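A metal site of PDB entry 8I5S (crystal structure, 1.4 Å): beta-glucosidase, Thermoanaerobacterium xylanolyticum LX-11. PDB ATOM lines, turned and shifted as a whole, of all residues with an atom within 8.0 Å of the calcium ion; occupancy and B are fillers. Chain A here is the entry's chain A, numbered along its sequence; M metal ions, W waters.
The side-chain carboxylate (OD2) of Asp 564 lies within hydrogen-bond range of the side-chain hydroxyl (OG1) of Thr 585, at 3.0 Å. The side-chain carboxylate (OE2) of Glu 630 lies close to the side-chain carboxylate (OD2) of Asp 564 (2.6 Å). O of Asp 564 sits at hydrogen-bond distance from ND2 of Asn 626, 2.8 Å away. OD1 of Asp 568 sits close to N of Lys 561, at 2.8 Å. The backbone NH (N) of Asp 568 sits at hydrogen-bond distance from the backbone carbonyl oxygen (O) of Met 559, at 3.0 Å. The backbone NH of Asn 563 lies close to the side-chain carboxylate of Asp 560, 3.2 Å away. OD2 of Asp 560 is in hydrogen-bond range of N of Gly 565 (2.8 Å).
Five residues have an atom within 4 Å of the calcium ion: Asp 560, Asp 562, Asp 564, Ile 566 and Asp 568. The nearest printed residue that does not touch the calcium ion is Lys 561 (4.2 Å).
The calcium ion is bound by OD1 of Asp 564 (2.3 Å), OD1 of Asp 568 (2.3 Å), O of Ile 566 (2.3 Å), water W1 (2.4 Å), OD1 of Asp 560 (2.4 Å) and OD1 of Asp 562 (2.4 Å). The calcium ion has six donor atoms within binding distance.
Water W1 lies within hydrogen-bond range of OG1 of Thr 585 (2.7 Å), O of Pro 567 (3.1 Å) and OD2 of Asp 568 (3.4 Å).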
ATOM      1  N   LYS A 557     -23.261   1.617  20.456  1.00  0.00           N
ATOM      2  CA  LYS A 557     -22.502   1.089  21.607  1.00  0.00           C
ATOM      3  C   LYS A 557     -21.698   2.190  22.297  1.00  0.00           C
ATOM      4  O   LYS A 557     -21.584   2.195  23.521  1.00  0.00           O
ATOM      5  CB  LYS A 557     -21.586  -0.044  21.163  1.00  0.00           C
ATOM      6  CG  LYS A 557     -20.798  -0.740  22.270  1.00  0.00           C
ATOM      7  CD  LYS A 557     -21.707  -1.230  23.380  1.00  0.00           C
ATOM      8  CE  LYS A 557     -21.223  -2.505  24.040  1.00  0.00           C
ATOM      9  NZ  LYS A 557     -19.937  -2.346  24.734  1.00  0.00           N
ATOM     10  N   MET A 559     -22.576   5.078  22.931  1.00  0.00           N
ATOM     11  CA  MET A 559     -23.470   5.871  23.783  1.00  0.00           C
ATOM     12  C   MET A 559     -23.778   5.213  25.120  1.00  0.00           C
ATOM     13  O   MET A 559     -24.563   5.721  25.903  1.00  0.00           O
ATOM     14  CB  MET A 559     -24.768   6.173  23.027  1.00  0.00           C
ATOM     15  CG  MET A 559     -24.502   7.019  21.802  1.00  0.00           C
ATOM     16  SD  MET A 559     -25.988   7.179  20.790  1.00  0.00           S
ATOM     17  CE  MET A 559     -25.343   8.291  19.537  1.00  0.00           C
ATOM     18  N   ASP A 560     -23.145   4.075  25.396  1.00  0.00           N
ATOM     19  CA  ASP A 560     -23.141   3.493  26.728  1.00  0.00           C
ATOM     20  C   ASP A 560     -22.183   4.327  27.592  1.00  0.00           C
ATOM     21  O   ASP A 560     -20.997   4.316  27.349  1.00  0.00           O
ATOM     22  CB  ASP A 560     -22.684   2.040  26.640  1.00  0.00           C
ATOM     23  CG  ASP A 560     -22.625   1.339  27.982  1.00  0.00           C
ATOM     24  OD1 ASP A 560     -23.173   1.845  28.975  1.00  0.00           O
ATOM     25  OD2 ASP A 560     -22.034   0.246  28.026  1.00  0.00           O
ATOM     26  N   LYS A 561     -22.723   5.039  28.574  1.00  0.00           N
ATOM     27  CA  LYS A 561     -21.915   5.938  29.411  1.00  0.00           C
ATOM     28  C   LYS A 561     -21.292   5.223  30.607  1.00  0.00           C
ATOM     29  O   LYS A 561     -20.178   5.573  31.010  1.00  0.00           O
ATOM     30  CB  LYS A 561     -22.770   7.119  29.886  1.00  0.00           C
ATOM     31  CG  LYS A 561     -23.033   8.125  28.784  1.00  0.00           C
ATOM     32  CD  LYS A 561     -24.284   8.958  29.025  1.00  0.00           C
ATOM     33  CE  LYS A 561     -24.115   9.971  30.146  1.00  0.00           C
ATOM     34  NZ  LYS A 561     -25.288  10.878  30.198  1.00  0.00           N
ATOM     35  N   ASP A 562     -21.977   4.227  31.143  1.00  0.00           N
ATOM     36  CA  ASP A 562     -21.608   3.602  32.423  1.00  0.00           C
ATOM     37  C   ASP A 562     -21.104   2.163  32.305  1.00  0.00           C
ATOM     38  O   ASP A 562     -21.002   1.461  33.316  1.00  0.00           O
ATOM     39  CB  ASP A 562     -22.799   3.691  33.390  1.00  0.00           C
ATOM     40  CG  ASP A 562     -23.963   2.819  32.968  1.00  0.00           C
ATOM     41  OD1 ASP A 562     -24.066   2.492  31.764  1.00  0.00           O
ATOM     42  OD2 ASP A 562     -24.791   2.486  33.831  1.00  0.00           O
ATOM     43  N   ASN A 563     -20.800   1.729  31.085  1.00  0.00           N
ATOM     44  CA  ASN A 563     -20.249   0.397  30.815  1.00  0.00           C
ATOM     45  C   ASN A 563     -21.110  -0.785  31.303  1.00  0.00           C
ATOM     46  O   ASN A 563     -20.588  -1.834  31.689  1.00  0.00           O
ATOM     47  CB  ASN A 563     -18.808   0.294  31.371  1.00  0.00           C
ATOM     48  CG  ASN A 563     -17.967  -0.770  30.658  1.00  0.00           C
ATOM     49  OD1 ASN A 563     -18.373  -1.344  29.645  1.00  0.00           O
ATOM     50  ND2 ASN A 563     -16.783  -1.028  31.195  1.00  0.00           N
ATOM     51  N   ASP A 564     -22.436  -0.622  31.265  1.00  0.00           N
ATOM     52  CA  ASP A 564     -23.355  -1.754  31.506  1.00  0.00           C
ATOM     53  C   ASP A 564     -23.707  -2.495  30.198  1.00  0.00           C
ATOM     54  O   ASP A 564     -24.511  -3.441  30.223  1.00  0.00           O
ATOM     55  CB  ASP A 564     -24.606  -1.286  32.261  1.00  0.00           C
ATOM     56  CG  ASP A 564     -25.653  -0.615  31.369  1.00  0.00           C
ATOM     57  OD1 ASP A 564     -25.295  -0.138  30.295  1.00  0.00           O
ATOM     58  OD2 ASP A 564     -26.817  -0.533  31.779  1.00  0.00           O
ATOM     59  N   GLY A 565     -23.125  -2.075  29.077  1.00  0.00           N
ATOM     60  CA  GLY A 565     -23.309  -2.719  27.774  1.00  0.00           C
ATOM     61  C   GLY A 565     -24.552  -2.254  27.007  1.00  0.00           C
ATOM     62  O   GLY A 565     -24.840  -2.813  25.953  1.00  0.00           O
ATOM     63  N   ILE A 566     -25.229  -1.210  27.504  1.00  0.00           N
ATOM     64  CA  ILE A 566     -26.494  -0.726  26.921  1.00  0.00           C
ATOM     65  C   ILE A 566     -26.364   0.784  26.710  1.00  0.00           C
ATOM     66  O   ILE A 566     -25.905   1.498  27.612  1.00  0.00           O
ATOM     67  CB  ILE A 566     -27.681  -0.991  27.867  1.00  0.00           C
ATOM     68  CG1 ILE A 566     -27.712  -2.465  28.311  1.00  0.00           C
ATOM     69  CG2 ILE A 566     -29.003  -0.619  27.196  1.00  0.00           C
ATOM     70  CD1 ILE A 566     -28.704  -2.774  29.398  1.00  0.00           C
ATOM     71  N   PRO A 567     -26.775   1.300  25.536  1.00  0.00           N
ATOM     72  CA  PRO A 567     -26.736   2.754  25.389  1.00  0.00           C
ATOM     73  C   PRO A 567     -27.593   3.454  26.431  1.00  0.00           C
ATOM     74  O   PRO A 567     -28.643   2.931  26.813  1.00  0.00           O
ATOM     75  CB  PRO A 567     -27.280   2.994  23.967  1.00  0.00           C
ATOM     76  CG  PRO A 567     -27.993   1.744  23.589  1.00  0.00           C
ATOM     77  CD  PRO A 567     -27.329   0.628  24.335  1.00  0.00           C
ATOM     78  N   ASP A 568     -27.138   4.616  26.911  1.00  0.00           N
ATOM     79  CA  ASP A 568     -27.859   5.389  27.937  1.00  0.00           C
ATOM     80  C   ASP A 568     -28.741   6.449  27.312  1.00  0.00           C
ATOM     81  O   ASP A 568     -28.262   7.290  26.574  1.00  0.00           O
ATOM     82  CB  ASP A 568     -26.882   6.123  28.867  1.00  0.00           C
ATOM     83  CG  ASP A 568     -26.197   5.188  29.844  1.00  0.00           C
ATOM     84  OD1 ASP A 568     -25.350   4.383  29.376  1.00  0.00           O
ATOM     85  OD2 ASP A 568     -26.542   5.223  31.045  1.00  0.00           O
ATOM     86  N   ASN A 569     -30.040   6.426  27.652  1.00  0.00           N
ATOM     87  CA  ASN A 569     -30.921   7.540  27.340  1.00  0.00           C
ATOM     88  C   ASN A 569     -30.460   8.730  28.205  1.00  0.00           C
ATOM     89  O   ASN A 569     -30.018   8.543  29.334  1.00  0.00           O
ATOM     90  CB  ASN A 569     -32.391   7.195  27.606  1.00  0.00           C
ATOM     91  CG  ASN A 569     -32.918   6.131  26.647  1.00  0.00           C
ATOM     92  OD1 ASN A 569     -33.025   4.962  27.011  1.00  0.00           O
ATOM     93  ND2 ASN A 569     -33.235   6.538  25.431  1.00  0.00           N
ATOM     94  N   GLY A 584     -30.917   6.772  31.501  1.00  0.00           N
ATOM     95  CA  GLY A 584     -30.197   5.547  31.793  1.00  0.00           C
ATOM     96  C   GLY A 584     -30.638   4.428  30.877  1.00  0.00           C
ATOM     97  O   GLY A 584     -30.749   4.614  29.661  1.00  0.00           O
ATOM     98  N   THR A 585     -30.849   3.240  31.434  1.00  0.00           N
ATOM     99  CA  THR A 585     -31.341   2.108  30.651  1.00  0.00           C
ATOM    100  C   THR A 585     -32.853   2.155  30.651  1.00  0.00           C
ATOM    101  O   THR A 585     -33.463   2.153  31.709  1.00  0.00           O
ATOM    102  CB  THR A 585     -30.854   0.761  31.213  1.00  0.00           C
ATOM    103  OG1 THR A 585     -29.422   0.698  31.128  1.00  0.00           O
ATOM    104  CG2 THR A 585     -31.456  -0.416  30.430  1.00  0.00           C
ATOM    105  N   TRP A 593     -32.337  -2.568  21.612  1.00  0.00           N
ATOM    106  CA  TRP A 593     -30.907  -2.841  21.518  1.00  0.00           C
ATOM    107  C   TRP A 593     -30.589  -4.337  21.601  1.00  0.00           C
ATOM    108  O   TRP A 593     -29.854  -4.867  20.772  1.00  0.00           O
ATOM    109  CB  TRP A 593     -30.191  -2.049  22.620  1.00  0.00           C
ATOM    110  CG  TRP A 593     -28.731  -2.344  22.860  1.00  0.00           C
ATOM    111  CD1 TRP A 593     -28.193  -2.852  24.020  1.00  0.00           C
ATOM    112  CD2 TRP A 593     -27.634  -2.072  21.989  1.00  0.00           C
ATOM    113  NE1 TRP A 593     -26.825  -2.935  23.900  1.00  0.00           N
ATOM    114  CE2 TRP A 593     -26.459  -2.474  22.652  1.00  0.00           C
ATOM    115  CE3 TRP A 593     -27.518  -1.553  20.694  1.00  0.00           C
ATOM    116  CZ2 TRP A 593     -25.173  -2.351  22.072  1.00  0.00           C
ATOM    117  CZ3 TRP A 593     -26.265  -1.444  20.110  1.00  0.00           C
ATOM    118  CH2 TRP A 593     -25.103  -1.840  20.815  1.00  0.00           C
ATOM    119  N   ASN A 626     -27.604  -7.420  32.289  1.00  0.00           N
ATOM    120  CA  ASN A 626     -27.771  -6.138  32.957  1.00  0.00           C
ATOM    121  C   ASN A 626     -29.167  -5.518  32.777  1.00  0.00           C
ATOM    122  O   ASN A 626     -29.669  -4.864  33.689  1.00  0.00           O
ATOM    123  CB  ASN A 626     -26.681  -5.173  32.513  1.00  0.00           C
ATOM    124  CG  ASN A 626     -25.336  -5.517  33.111  1.00  0.00           C
ATOM    125  OD1 ASN A 626     -25.277  -6.103  34.205  1.00  0.00           O
ATOM    126  ND2 ASN A 626     -24.260  -5.158  32.443  1.00  0.00           N
ATOM    127  N   GLU A 630     -31.303  -4.611  36.035  1.00  0.00           N
ATOM    128  CA  GLU A 630     -31.658  -3.212  36.224  1.00  0.00           C
ATOM    129  C   GLU A 630     -33.155  -2.951  36.208  1.00  0.00           C
ATOM    130  O   GLU A 630     -33.632  -2.056  36.906  1.00  0.00           O
ATOM    131  CB  GLU A 630     -30.997  -2.350  35.133  1.00  0.00           C
ATOM    132  CG  GLU A 630     -29.491  -2.198  35.273  1.00  0.00           C
ATOM    133  CD  GLU A 630     -28.822  -1.728  33.989  1.00  0.00           C
ATOM    134  OE1 GLU A 630     -29.535  -1.201  33.102  1.00  0.00           O
ATOM    135  OE2 GLU A 630     -27.583  -1.879  33.848  1.00  0.00           O
ATOM    136  N   THR A 641     -34.067   3.353  34.365  1.00  0.00           N
ATOM    137  CA  THR A 641     -33.324   3.272  35.633  1.00  0.00           C
ATOM    138  C   THR A 641     -33.164   4.592  36.387  1.00  0.00           C
ATOM    139  O   THR A 641     -32.862   4.554  37.580  1.00  0.00           O
ATOM    140  CB  THR A 641     -31.933   2.679  35.397  1.00  0.00           C
ATOM    141  OG1 THR A 641     -31.251   3.435  34.389  1.00  0.00           O
ATOM    142  CG2 THR A 641     -32.031   1.239  34.985  1.00  0.00           C
ATOM    143  N   GLU A 642     -33.344   5.733  35.726  1.00  0.00           N
ATOM    144  CA  GLU A 642     -33.008   7.018  36.365  1.00  0.00           C
ATOM    145  C   GLU A 642     -34.081   8.129  36.396  1.00  0.00           C
ATOM    146  O   GLU A 642     -33.867   9.143  37.058  1.00  0.00           O
ATOM    147  CB  GLU A 642     -31.728   7.560  35.735  1.00  0.00           C
ATOM    148  CG  GLU A 642     -30.511   6.693  35.993  1.00  0.00           C
ATOM    149  CD  GLU A 642     -29.247   7.256  35.375  1.00  0.00           C
ATOM    150  OE1 GLU A 642     -29.066   8.490  35.387  1.00  0.00           O
ATOM    151  OE2 GLU A 642     -28.416   6.465  34.876  1.00  0.00           O
HETATM  152 CA    CA M   1     -25.389   2.105  29.810  1.00  0.00          CA
HETATM  153  O   HOH W   1     -27.744   2.309  29.747  1.00  0.00           O
HETATM  154  O   HOH W   2     -27.277   2.786  32.510  1.00  0.00           O
